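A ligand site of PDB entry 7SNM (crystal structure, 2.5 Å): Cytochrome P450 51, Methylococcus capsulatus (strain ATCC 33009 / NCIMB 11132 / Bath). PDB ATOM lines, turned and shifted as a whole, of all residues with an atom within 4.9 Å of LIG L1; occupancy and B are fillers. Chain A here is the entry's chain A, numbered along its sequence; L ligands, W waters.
Residues that only touch LIG L1: Leu 103 (3.6 Å), Leu 157 (3.7 Å), Ala 257 (3.1 Å), Gly 258 (3.9 Å), Thr 261 (3.3 Å), Ser 262 (3.6 Å), Pro 321 (3.5 Å), Leu 322 (3.8 Å), Leu 325 (3.8 Å), Ala 386 (3.3 Å), Phe 387 (3.5 Å), Gly 388 (3.7 Å), Lys 393 (3.3 Å), Ser 395 (3.4 Å), Gly 396 (3.8 Å), Phe 399 (3.8 Å) and Ala 400 (3.6 Å).
Hydrophobic or aromatic side chains that line LIG L1: Tyr 79, Leu 103, Leu 157, Ala 257, Pro 321, Leu 322, Leu 325, Phe 387, His 392, Phe 399 and Ala 400.
23 residues have an atom within 4 Å of LIG L1: Gln 75, Tyr 79, Lys 99, Leu 103, Leu 157, Ala 257, Gly 258, Thr 261, Ser 262, Pro 321, Leu 322, Leu 325, Arg 327, Ala 386, Phe 387, Gly 388, His 392, Lys 393, Cys 394, Ser 395, Gly 396, Phe 399 and Ala 400.
Along chain A the residues within 4 Å of LIG L1 span positions 75 to 400.
The nearest printed residue that does not touch LIG L1 is Leu 106 (4.03 Å).
The backbone NH (N) of Cys 394 sits at hydrogen-bond distance from the backbone carbonyl oxygen (O) of Phe 387 (2.8 Å).
SG of Cys 394 lies close to N of Gly 396 (3.4 Å).
The backbone carbonyl oxygen of Ala 257 sits at hydrogen-bond distance from the side-chain hydroxyl of Thr 261 (2.7 Å).
The side-chain hydroxyl of Thr 261 sits at hydrogen-bond distance from the side-chain hydroxyl of Ser 262, at 2.8 Å.
Water W1 bridges O2 of LIG L1 (2.7 Å) and O of His 392 (3.3 Å).
Water W2 lies within hydrogen-bond range of OE1 of Gln 75 (2.7 Å), O of His 392 (2.7 Å) and O4 of LIG L1 (2.9 Å).
The side-chain sulfur (SG) of Cys 394 is bound to an iron atom (FE1) of LIG L1 (2.3 Å).
An oxygen (O2) of LIG L1 is in salt-bridge range of the guanidinium group (NH2) of Arg 327 (2.9 Å).
The side-chain hydroxyl of Tyr 79 is in hydrogen-bond range of an oxygen (O1) of LIG L1, 2.9 Å away.
An oxygen (O1) of LIG L1 lies close to the side-chain amide oxygen of Gln 75, 3.0 Å away.
A ring nitrogen (ND1) of His 392 sits at hydrogen-bond distance from an oxygen (O4) of LIG L1.
NZ of Lys 99 is in salt-bridge range of O4 of LIG L1.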
ATOM      1  N   GLN A  75     -37.721  21.313  33.676  1.00  0.00           N
ATOM      2  CA  GLN A  75     -36.495  20.748  33.059  1.00  0.00           C
ATOM      3  C   GLN A  75     -35.991  19.592  33.935  1.00  0.00           C
ATOM      4  O   GLN A  75     -35.312  18.701  33.398  1.00  0.00           O
ATOM      5  CB  GLN A  75     -35.413  21.827  32.958  1.00  0.00           C
ATOM      6  CG  GLN A  75     -35.689  22.881  31.900  1.00  0.00           C
ATOM      7  CD  GLN A  75     -34.627  23.958  31.902  1.00  0.00           C
ATOM      8  OE1 GLN A  75     -33.905  24.149  30.923  1.00  0.00           O
ATOM      9  NE2 GLN A  75     -34.547  24.694  33.004  1.00  0.00           N
ATOM     10  N   TYR A  79     -34.114  15.989  32.628  1.00  0.00           N
ATOM     11  CA  TYR A  79     -32.653  16.089  32.412  1.00  0.00           C
ATOM     12  C   TYR A  79     -31.883  15.335  33.513  1.00  0.00           C
ATOM     13  O   TYR A  79     -30.660  15.563  33.628  1.00  0.00           O
ATOM     14  CB  TYR A  79     -32.235  17.555  32.298  1.00  0.00           C
ATOM     15  CG  TYR A  79     -32.680  18.265  31.038  1.00  0.00           C
ATOM     16  CD1 TYR A  79     -33.007  17.581  29.878  1.00  0.00           C
ATOM     17  CD2 TYR A  79     -32.696  19.643  30.991  1.00  0.00           C
ATOM     18  CE1 TYR A  79     -33.345  18.257  28.709  1.00  0.00           C
ATOM     19  CE2 TYR A  79     -33.038  20.328  29.845  1.00  0.00           C
ATOM     20  CZ  TYR A  79     -33.363  19.630  28.686  1.00  0.00           C
ATOM     21  OH  TYR A  79     -33.711  20.345  27.568  1.00  0.00           O
ATOM     22  N   LYS A  99     -30.146  25.927  42.412  1.00  0.00           N
ATOM     23  CA  LYS A  99     -29.845  25.915  40.961  1.00  0.00           C
ATOM     24  C   LYS A  99     -29.588  27.356  40.496  1.00  0.00           C
ATOM     25  O   LYS A  99     -28.540  27.611  39.871  1.00  0.00           O
ATOM     26  CB  LYS A  99     -30.996  25.268  40.179  1.00  0.00           C
ATOM     27  CG  LYS A  99     -30.753  25.164  38.675  1.00  0.00           C
ATOM     28  CD  LYS A  99     -32.004  24.909  37.865  1.00  0.00           C
ATOM     29  CE  LYS A  99     -32.600  26.144  37.230  1.00  0.00           C
ATOM     30  NZ  LYS A  99     -32.380  26.132  35.759  1.00  0.00           N
ATOM     31  N   LEU A 103     -26.245  28.980  38.846  1.00  0.00           N
ATOM     32  CA  LEU A 103     -26.220  29.685  37.534  1.00  0.00           C
ATOM     33  C   LEU A 103     -25.745  31.123  37.756  1.00  0.00           C
ATOM     34  O   LEU A 103     -24.918  31.588  36.948  1.00  0.00           O
ATOM     35  CB  LEU A 103     -27.608  29.629  36.866  1.00  0.00           C
ATOM     36  CG  LEU A 103     -28.037  28.251  36.348  1.00  0.00           C
ATOM     37  CD1 LEU A 103     -29.077  28.354  35.241  1.00  0.00           C
ATOM     38  CD2 LEU A 103     -26.865  27.436  35.831  1.00  0.00           C
ATOM     39  N   LEU A 106     -21.841  32.064  37.572  1.00  0.00           N
ATOM     40  CA  LEU A 106     -21.149  32.237  36.262  1.00  0.00           C
ATOM     41  C   LEU A 106     -21.496  33.613  35.668  1.00  0.00           C
ATOM     42  O   LEU A 106     -20.637  34.163  34.958  1.00  0.00           O
ATOM     43  CB  LEU A 106     -21.577  31.130  35.284  1.00  0.00           C
ATOM     44  CG  LEU A 106     -21.017  31.259  33.870  1.00  0.00           C
ATOM     45  CD1 LEU A 106     -19.503  31.302  33.899  1.00  0.00           C
ATOM     46  CD2 LEU A 106     -21.540  30.139  32.989  1.00  0.00           C
ATOM     47  N   MET A 107     -22.715  34.111  35.912  1.00  0.00           N
ATOM     48  CA  MET A 107     -23.244  35.351  35.294  1.00  0.00           C
ATOM     49  C   MET A 107     -22.184  36.462  35.366  1.00  0.00           C
ATOM     50  O   MET A 107     -21.953  37.122  34.355  1.00  0.00           O
ATOM     51  CB  MET A 107     -24.546  35.800  35.956  1.00  0.00           C
ATOM     52  CG  MET A 107     -25.758  34.951  35.605  1.00  0.00           C
ATOM     53  SD  MET A 107     -25.900  34.404  33.881  1.00  0.00           S
ATOM     54  CE  MET A 107     -27.008  33.001  34.009  1.00  0.00           C
ATOM     55  N   LEU A 110     -19.909  36.976  32.485  1.00  0.00           N
ATOM     56  CA  LEU A 110     -20.595  37.254  31.197  1.00  0.00           C
ATOM     57  C   LEU A 110     -20.832  38.754  31.031  1.00  0.00           C
ATOM     58  O   LEU A 110     -21.318  39.158  29.957  1.00  0.00           O
ATOM     59  CB  LEU A 110     -21.912  36.470  31.138  1.00  0.00           C
ATOM     60  CG  LEU A 110     -21.839  35.074  30.529  1.00  0.00           C
ATOM     61  CD1 LEU A 110     -20.795  34.220  31.225  1.00  0.00           C
ATOM     62  CD2 LEU A 110     -23.199  34.394  30.574  1.00  0.00           C
ATOM     63  N   LEU A 157     -13.664  31.845  31.337  1.00  0.00           N
ATOM     64  CA  LEU A 157     -14.786  31.809  32.313  1.00  0.00           C
ATOM     65  C   LEU A 157     -14.359  31.271  33.683  1.00  0.00           C
ATOM     66  O   LEU A 157     -15.053  31.615  34.659  1.00  0.00           O
ATOM     67  CB  LEU A 157     -15.907  30.972  31.688  1.00  0.00           C
ATOM     68  CG  LEU A 157     -16.438  31.498  30.351  1.00  0.00           C
ATOM     69  CD1 LEU A 157     -17.243  30.427  29.631  1.00  0.00           C
ATOM     70  CD2 LEU A 157     -17.270  32.761  30.551  1.00  0.00           C
ATOM     71  N   ALA A 257     -20.919  23.973  28.768  1.00  0.00           N
ATOM     72  CA  ALA A 257     -21.503  25.233  28.246  1.00  0.00           C
ATOM     73  C   ALA A 257     -20.525  25.884  27.256  1.00  0.00           C
ATOM     74  O   ALA A 257     -20.984  26.335  26.183  1.00  0.00           O
ATOM     75  CB  ALA A 257     -21.838  26.161  29.381  1.00  0.00           C
ATOM     76  N   GLY A 258     -19.247  26.014  27.635  1.00  0.00           N
ATOM     77  CA  GLY A 258     -18.297  26.877  26.902  1.00  0.00           C
ATOM     78  C   GLY A 258     -17.654  26.122  25.742  1.00  0.00           C
ATOM     79  O   GLY A 258     -17.115  26.787  24.838  1.00  0.00           O
ATOM     80  N   THR A 261     -20.804  22.806  23.556  1.00  0.00           N
ATOM     81  CA  THR A 261     -21.848  23.424  22.704  1.00  0.00           C
ATOM     82  C   THR A 261     -21.224  23.910  21.396  1.00  0.00           C
ATOM     83  O   THR A 261     -21.969  24.053  20.404  1.00  0.00           O
ATOM     84  CB  THR A 261     -22.511  24.638  23.380  1.00  0.00           C
ATOM     85  OG1 THR A 261     -21.526  25.636  23.609  1.00  0.00           O
ATOM     86  CG2 THR A 261     -23.196  24.301  24.687  1.00  0.00           C
ATOM     87  N   SER A 262     -19.912  24.201  21.417  1.00  0.00           N
ATOM     88  CA  SER A 262     -19.306  25.229  20.528  1.00  0.00           C
ATOM     89  C   SER A 262     -18.252  24.599  19.614  1.00  0.00           C
ATOM     90  O   SER A 262     -17.928  25.206  18.574  1.00  0.00           O
ATOM     91  CB  SER A 262     -18.731  26.364  21.317  1.00  0.00           C
ATOM     92  OG  SER A 262     -19.755  27.044  22.014  1.00  0.00           O
ATOM     93  N   THR A 265     -19.826  23.740  16.122  1.00  0.00           N
ATOM     94  CA  THR A 265     -20.405  24.865  15.332  1.00  0.00           C
ATOM     95  C   THR A 265     -19.263  25.780  14.892  1.00  0.00           C
ATOM     96  O   THR A 265     -19.379  26.344  13.782  1.00  0.00           O
ATOM     97  CB  THR A 265     -21.579  25.524  16.048  1.00  0.00           C
ATOM     98  OG1 THR A 265     -21.113  26.091  17.271  1.00  0.00           O
ATOM     99  CG2 THR A 265     -22.691  24.530  16.356  1.00  0.00           C
ATOM    100  N   LEU A 316     -25.899  27.692  12.733  1.00  0.00           N
ATOM    101  CA  LEU A 316     -26.754  27.279  13.871  1.00  0.00           C
ATOM    102  C   LEU A 316     -28.156  26.864  13.387  1.00  0.00           C
ATOM    103  O   LEU A 316     -28.773  26.027  14.083  1.00  0.00           O
ATOM    104  CB  LEU A 316     -26.836  28.402  14.911  1.00  0.00           C
ATOM    105  CG  LEU A 316     -25.584  28.574  15.761  1.00  0.00           C
ATOM    106  CD1 LEU A 316     -25.739  29.763  16.697  1.00  0.00           C
ATOM    107  CD2 LEU A 316     -25.256  27.311  16.540  1.00  0.00           C
ATOM    108  N   PRO A 321     -26.471  22.282  17.586  1.00  0.00           N
ATOM    109  CA  PRO A 321     -25.843  21.180  18.305  1.00  0.00           C
ATOM    110  C   PRO A 321     -26.800  20.466  19.274  1.00  0.00           C
ATOM    111  O   PRO A 321     -26.748  19.252  19.334  1.00  0.00           O
ATOM    112  CB  PRO A 321     -24.671  21.827  19.052  1.00  0.00           C
ATOM    113  CG  PRO A 321     -25.041  23.279  19.147  1.00  0.00           C
ATOM    114  CD  PRO A 321     -25.922  23.593  17.958  1.00  0.00           C
ATOM    115  N   LEU A 322     -27.669  21.206  19.984  1.00  0.00           N
ATOM    116  CA  LEU A 322     -28.681  20.592  20.883  1.00  0.00           C
ATOM    117  C   LEU A 322     -29.989  20.439  20.099  1.00  0.00           C
ATOM    118  O   LEU A 322     -30.638  21.458  19.813  1.00  0.00           O
ATOM    119  CB  LEU A 322     -28.894  21.448  22.139  1.00  0.00           C
ATOM    120  CG  LEU A 322     -27.639  22.020  22.787  1.00  0.00           C
ATOM    121  CD1 LEU A 322     -27.945  22.544  24.189  1.00  0.00           C
ATOM    122  CD2 LEU A 322     -26.542  20.972  22.875  1.00  0.00           C
ATOM    123  N   LEU A 325     -34.600  19.374  23.228  1.00  0.00           N
ATOM    124  CA  LEU A 325     -34.854  20.062  24.526  1.00  0.00           C
ATOM    125  C   LEU A 325     -36.144  19.464  25.089  1.00  0.00           C
ATOM    126  O   LEU A 325     -37.030  19.114  24.293  1.00  0.00           O
ATOM    127  CB  LEU A 325     -34.991  21.563  24.276  1.00  0.00           C
ATOM    128  CG  LEU A 325     -33.905  22.191  23.414  1.00  0.00           C
ATOM    129  CD1 LEU A 325     -34.080  23.704  23.383  1.00  0.00           C
ATOM    130  CD2 LEU A 325     -32.519  21.860  23.924  1.00  0.00           C
ATOM    131  N   ARG A 327     -39.018  18.857  28.610  1.00  0.00           N
ATOM    132  CA  ARG A 327     -39.610  19.146  29.949  1.00  0.00           C
ATOM    133  C   ARG A 327     -40.548  18.006  30.350  1.00  0.00           C
ATOM    134  O   ARG A 327     -41.229  17.464  29.457  1.00  0.00           O
ATOM    135  CB  ARG A 327     -40.416  20.450  29.913  1.00  0.00           C
ATOM    136  CG  ARG A 327     -39.802  21.578  29.090  1.00  0.00           C
ATOM    137  CD  ARG A 327     -38.937  22.481  29.933  1.00  0.00           C
ATOM    138  NE  ARG A 327     -38.362  23.587  29.178  1.00  0.00           N
ATOM    139  CZ  ARG A 327     -37.160  23.589  28.606  1.00  0.00           C
ATOM    140  NH1 ARG A 327     -36.420  22.493  28.584  1.00  0.00           N
ATOM    141  NH2 ARG A 327     -36.722  24.706  28.055  1.00  0.00           N
ATOM    142  N   GLN A 385     -34.340  28.610  16.911  1.00  0.00           N
ATOM    143  CA  GLN A 385     -34.312  28.233  18.350  1.00  0.00           C
ATOM    144  C   GLN A 385     -33.086  27.390  18.692  1.00  0.00           C
ATOM    145  O   GLN A 385     -33.155  26.638  19.681  1.00  0.00           O
ATOM    146  CB  GLN A 385     -35.596  27.508  18.750  1.00  0.00           C
ATOM    147  CG  GLN A 385     -35.903  26.298  17.882  1.00  0.00           C
ATOM    148  CD  GLN A 385     -37.239  25.676  18.224  1.00  0.00           C
ATOM    149  OE1 GLN A 385     -37.349  24.790  19.064  1.00  0.00           O
ATOM    150  NE2 GLN A 385     -38.278  26.146  17.562  1.00  0.00           N
ATOM    151  N   ALA A 386     -31.916  27.703  18.105  1.00  0.00           N
ATOM    152  CA  ALA A 386     -30.645  27.047  18.461  1.00  0.00           C
ATOM    153  C   ALA A 386     -30.306  27.330  19.937  1.00  0.00           C
ATOM    154  O   ALA A 386     -29.635  26.470  20.553  1.00  0.00           O
ATOM    155  CB  ALA A 386     -29.548  27.506  17.535  1.00  0.00           C
ATOM    156  N   PHE A 387     -30.728  28.475  20.482  1.00  0.00           N
ATOM    157  CA  PHE A 387     -30.425  28.909  21.868  1.00  0.00           C
ATOM    158  C   PHE A 387     -31.665  28.741  22.755  1.00  0.00           C
ATOM    159  O   PHE A 387     -31.650  29.248  23.898  1.00  0.00           O
ATOM    160  CB  PHE A 387     -29.959  30.366  21.904  1.00  0.00           C
ATOM    161  CG  PHE A 387     -28.582  30.596  21.339  1.00  0.00           C
ATOM    162  CD1 PHE A 387     -27.490  29.946  21.898  1.00  0.00           C
ATOM    163  CD2 PHE A 387     -28.386  31.416  20.244  1.00  0.00           C
ATOM    164  CE1 PHE A 387     -26.224  30.118  21.359  1.00  0.00           C
ATOM    165  CE2 PHE A 387     -27.116  31.591  19.719  1.00  0.00           C
ATOM    166  CZ  PHE A 387     -26.036  30.953  20.279  1.00  0.00           C
ATOM    167  N   GLY A 388     -32.693  28.064  22.252  1.00  0.00           N
ATOM    168  CA  GLY A 388     -33.965  27.883  22.965  1.00  0.00           C
ATOM    169  C   GLY A 388     -34.802  29.149  22.949  1.00  0.00           C
ATOM    170  O   GLY A 388     -34.716  29.888  21.942  1.00  0.00           O
ATOM    171  N   ARG A 391     -38.351  31.573  29.341  1.00  0.00           N
ATOM    172  CA  ARG A 391     -37.617  31.811  30.615  1.00  0.00           C
ATOM    173  C   ARG A 391     -36.217  31.195  30.525  1.00  0.00           C
ATOM    174  O   ARG A 391     -35.255  31.882  30.927  1.00  0.00           O
ATOM    175  CB  ARG A 391     -38.381  31.238  31.812  1.00  0.00           C
ATOM    176  CG  ARG A 391     -39.166  32.277  32.600  1.00  0.00           C
ATOM    177  CD  ARG A 391     -40.305  31.665  33.402  1.00  0.00           C
ATOM    178  NE  ARG A 391     -41.331  31.088  32.543  1.00  0.00           N
ATOM    179  CZ  ARG A 391     -42.372  31.737  32.044  1.00  0.00           C
ATOM    180  NH1 ARG A 391     -42.578  33.014  32.321  1.00  0.00           N
ATOM    181  NH2 ARG A 391     -43.220  31.106  31.258  1.00  0.00           N
ATOM    182  N   HIS A 392     -36.084  29.966  30.003  1.00  0.00           N
ATOM    183  CA  HIS A 392     -34.859  29.138  30.180  1.00  0.00           C
ATOM    184  C   HIS A 392     -34.033  29.139  28.889  1.00  0.00           C
ATOM    185  O   HIS A 392     -33.147  28.269  28.748  1.00  0.00           O
ATOM    186  CB  HIS A 392     -35.229  27.760  30.745  1.00  0.00           C
ATOM    187  CG  HIS A 392     -35.700  27.851  32.155  1.00  0.00           C
ATOM    188  ND1 HIS A 392     -34.957  28.468  33.139  1.00  0.00           N
ATOM    189  CD2 HIS A 392     -36.900  27.588  32.700  1.00  0.00           C
ATOM    190  CE1 HIS A 392     -35.652  28.508  34.259  1.00  0.00           C
ATOM    191  NE2 HIS A 392     -36.859  27.984  34.013  1.00  0.00           N
ATOM    192  N   LYS A 393     -34.172  30.207  28.100  1.00  0.00           N
ATOM    193  CA  LYS A 393     -33.313  30.524  26.937  1.00  0.00           C
ATOM    194  C   LYS A 393     -31.833  30.442  27.341  1.00  0.00           C
ATOM    195  O   LYS A 393     -31.545  30.721  28.521  1.00  0.00           O
ATOM    196  CB  LYS A 393     -33.666  31.911  26.395  1.00  0.00           C
ATOM    197  CG  LYS A 393     -33.086  32.256  25.029  1.00  0.00           C
ATOM    198  CD  LYS A 393     -33.514  33.622  24.543  1.00  0.00           C
ATOM    199  CE  LYS A 393     -33.464  33.797  23.039  1.00  0.00           C
ATOM    200  NZ  LYS A 393     -32.066  33.771  22.539  1.00  0.00           N
ATOM    201  N   CYS A 394     -30.930  30.140  26.408  1.00  0.00           N
ATOM    202  CA  CYS A 394     -29.471  30.230  26.679  1.00  0.00           C
ATOM    203  C   CYS A 394     -29.161  31.613  27.292  1.00  0.00           C
ATOM    204  O   CYS A 394     -29.511  32.611  26.644  1.00  0.00           O
ATOM    205  CB  CYS A 394     -28.625  30.072  25.424  1.00  0.00           C
ATOM    206  SG  CYS A 394     -26.856  29.848  25.752  1.00  0.00           S
ATOM    207  N   SER A 395     -28.494  31.659  28.447  1.00  0.00           N
ATOM    208  CA  SER A 395     -28.005  32.938  29.049  1.00  0.00           C
ATOM    209  C   SER A 395     -26.523  33.167  28.714  1.00  0.00           C
ATOM    210  O   SER A 395     -25.977  34.147  29.249  1.00  0.00           O
ATOM    211  CB  SER A 395     -28.291  33.047  30.521  1.00  0.00           C
ATOM    212  OG  SER A 395     -27.832  31.905  31.222  1.00  0.00           O
ATOM    213  N   GLY A 396     -25.980  32.488  27.700  1.00  0.00           N
ATOM    214  CA  GLY A 396     -24.555  32.622  27.349  1.00  0.00           C
ATOM    215  C   GLY A 396     -24.323  32.804  25.857  1.00  0.00           C
ATOM    216  O   GLY A 396     -23.178  32.621  25.401  1.00  0.00           O
ATOM    217  N   PHE A 399     -21.546  35.384  24.722  1.00  0.00           N
ATOM    218  CA  PHE A 399     -20.167  34.845  24.830  1.00  0.00           C
ATOM    219  C   PHE A 399     -19.963  33.740  23.780  1.00  0.00           C
ATOM    220  O   PHE A 399     -18.852  33.625  23.244  1.00  0.00           O
ATOM    221  CB  PHE A 399     -19.867  34.320  26.236  1.00  0.00           C
ATOM    222  CG  PHE A 399     -18.538  33.622  26.327  1.00  0.00           C
ATOM    223  CD1 PHE A 399     -17.362  34.347  26.452  1.00  0.00           C
ATOM    224  CD2 PHE A 399     -18.442  32.245  26.163  1.00  0.00           C
ATOM    225  CE1 PHE A 399     -16.128  33.710  26.496  1.00  0.00           C
ATOM    226  CE2 PHE A 399     -17.209  31.620  26.177  1.00  0.00           C
ATOM    227  CZ  PHE A 399     -16.062  32.351  26.347  1.00  0.00           C
ATOM    228  N   ALA A 400     -20.986  32.914  23.533  1.00  0.00           N
ATOM    229  CA  ALA A 400     -20.912  31.796  22.568  1.00  0.00           C
ATOM    230  C   ALA A 400     -20.541  32.324  21.183  1.00  0.00           C
ATOM    231  O   ALA A 400     -19.550  31.856  20.594  1.00  0.00           O
ATOM    232  CB  ALA A 400     -22.226  31.045  22.533  1.00  0.00           C
HETATM  233  C1  LIG L   1     -29.185  26.987  27.956  1.00  0.00           C
HETATM  234  C2  LIG L   1     -27.725  26.304  23.376  1.00  0.00           C
HETATM  235  C3  LIG L   1     -23.384  28.215  24.477  1.00  0.00           C
HETATM  236  C4  LIG L   1     -24.856  28.832  29.061  1.00  0.00           C
HETATM  237  C5  LIG L   1     -29.136  26.652  26.615  1.00  0.00           C
HETATM  238  C6  LIG L   1     -30.214  26.067  25.922  1.00  0.00           C
HETATM  239  C7  LIG L   1     -29.819  25.889  24.635  1.00  0.00           C
HETATM  240  C8  LIG L   1     -28.491  26.337  24.534  1.00  0.00           C
HETATM  241  C9  LIG L   1     -30.644  25.313  23.515  1.00  0.00           C
HETATM  242  C10 LIG L   1     -31.577  25.769  26.506  1.00  0.00           C
HETATM  243  C11 LIG L   1     -31.728  24.290  26.854  1.00  0.00           C
HETATM  244  C12 LIG L   1     -33.131  24.082  27.379  1.00  0.00           C
HETATM  245  O1  LIG L   1     -33.400  23.153  28.168  1.00  0.00           O
HETATM  246  O2  LIG L   1     -34.050  24.853  27.013  1.00  0.00           O
HETATM  247  C13 LIG L   1     -26.419  26.777  23.346  1.00  0.00           C
HETATM  248  C14 LIG L   1     -25.661  26.703  22.144  1.00  0.00           C
HETATM  249  C15 LIG L   1     -24.435  27.239  22.419  1.00  0.00           C
HETATM  250  C16 LIG L   1     -24.484  27.632  23.849  1.00  0.00           C
HETATM  251  C17 LIG L   1     -26.147  26.154  20.836  1.00  0.00           C
HETATM  252  C18 LIG L   1     -23.299  27.404  21.504  1.00  0.00           C
HETATM  253  C19 LIG L   1     -23.473  27.818  20.253  1.00  0.00           C
HETATM  254  C20 LIG L   1     -23.392  28.578  25.824  1.00  0.00           C
HETATM  255  C21 LIG L   1     -22.324  29.135  26.539  1.00  0.00           C
HETATM  256  C22 LIG L   1     -22.745  29.304  27.842  1.00  0.00           C
HETATM  257  C23 LIG L   1     -24.076  28.832  27.925  1.00  0.00           C
HETATM  258  C24 LIG L   1     -20.985  29.478  25.934  1.00  0.00           C
HETATM  259  C25 LIG L   1     -21.993  29.864  28.994  1.00  0.00           C
HETATM  260  C26 LIG L   1     -20.823  30.465  28.853  1.00  0.00           C
HETATM  261  C27 LIG L   1     -26.170  28.356  29.065  1.00  0.00           C
HETATM  262  C28 LIG L   1     -26.919  28.343  30.327  1.00  0.00           C
HETATM  263  C29 LIG L   1     -28.136  27.849  30.029  1.00  0.00           C
HETATM  264  C30 LIG L   1     -28.078  27.536  28.593  1.00  0.00           C
HETATM  265  C31 LIG L   1     -26.454  28.835  31.679  1.00  0.00           C
HETATM  266  C32 LIG L   1     -29.280  27.630  30.998  1.00  0.00           C
HETATM  267  C33 LIG L   1     -30.320  28.745  30.915  1.00  0.00           C
HETATM  268  C34 LIG L   1     -31.241  28.657  32.105  1.00  0.00           C
HETATM  269  O3  LIG L   1     -31.411  29.660  32.823  1.00  0.00           O
HETATM  270  O4  LIG L   1     -31.824  27.592  32.418  1.00  0.00           O
HETATM  271  N1  LIG L   1     -28.077  26.810  25.754  1.00  0.00           N
HETATM  272  N2  LIG L   1     -25.699  27.333  24.329  1.00  0.00           N
HETATM  273  N3  LIG L   1     -24.451  28.391  26.674  1.00  0.00           N
HETATM  274  N4  LIG L   1     -26.894  27.869  28.059  1.00  0.00           N
HETATM  275 FE1  LIG L   1     -26.373  27.655  26.292  1.00  0.00          FE
HETATM  276  C1  LG2 L   2     -26.777  21.324  27.991  1.00  0.00           C
HETATM  277  C2  LG2 L   2     -25.911  20.252  27.443  1.00  0.00           C
HETATM  278  C3  LG2 L   2     -26.611  18.911  27.248  1.00  0.00           C
HETATM  279  C4  LG2 L   2     -27.998  19.165  26.673  1.00  0.00           C
HETATM  280  C5  LG2 L   2     -28.638  17.939  25.946  1.00  0.00           C
HETATM  281  C6  LG2 L   2     -28.837  16.733  26.883  1.00  0.00           C
HETATM  282  C7  LG2 L   2     -27.755  17.472  24.787  1.00  0.00           C
HETATM  283  C8  LG2 L   2     -29.999  18.370  25.385  1.00  0.00           C
HETATM  284  O1  LG2 L   2     -30.712  17.213  24.924  1.00  0.00           O
HETATM  285  C9  LG2 L   2     -30.879  19.117  26.365  1.00  0.00           C
HETATM  286  C10 LG2 L   2     -30.167  20.334  26.946  1.00  0.00           C
HETATM  287  C11 LG2 L   2     -28.878  19.944  27.694  1.00  0.00           C
HETATM  288  C12 LG2 L   2     -29.255  19.163  28.966  1.00  0.00           C
HETATM  289  C13 LG2 L   2     -28.117  21.201  28.150  1.00  0.00           C
HETATM  290  C14 LG2 L   2     -28.928  22.232  28.887  1.00  0.00           C
HETATM  291  C15 LG2 L   2     -28.172  23.360  29.607  1.00  0.00           C
HETATM  292  C16 LG2 L   2     -26.747  22.953  29.914  1.00  0.00           C
HETATM  293  C17 LG2 L   2     -26.731  21.769  30.904  1.00  0.00           C
HETATM  294  C18 LG2 L   2     -26.083  22.544  28.554  1.00  0.00           C
HETATM  295  C19 LG2 L   2     -26.211  23.654  27.482  1.00  0.00           C
HETATM  296  C20 LG2 L   2     -24.588  22.425  28.922  1.00  0.00           C
HETATM  297  C21 LG2 L   2     -24.384  23.448  30.060  1.00  0.00           C
HETATM  298  C22 LG2 L   2     -25.760  24.055  30.420  1.00  0.00           C
HETATM  299  C23 LG2 L   2     -25.827  24.512  31.884  1.00  0.00           C
HETATM  300  C24 LG2 L   2     -27.142  25.206  32.236  1.00  0.00           C
HETATM  301  C25 LG2 L   2     -24.625  25.421  32.193  1.00  0.00           C
HETATM  302  C26 LG2 L   2     -24.745  26.222  33.488  1.00  0.00           C
HETATM  303  C27 LG2 L   2     -23.445  26.857  33.869  1.00  0.00           C
HETATM  304  C28 LG2 L   2     -22.791  26.743  35.019  1.00  0.00           C
HETATM  305  C29 LG2 L   2     -21.315  26.988  35.137  1.00  0.00           C
HETATM  306  C30 LG2 L   2     -23.457  26.379  36.308  1.00  0.00           C
HETATM  307  O   HOH W   1     -35.022  27.259  26.214  1.00  0.00           O
HETATM  308  O   HOH W   2     -32.153  26.050  30.022  1.00  0.00           O
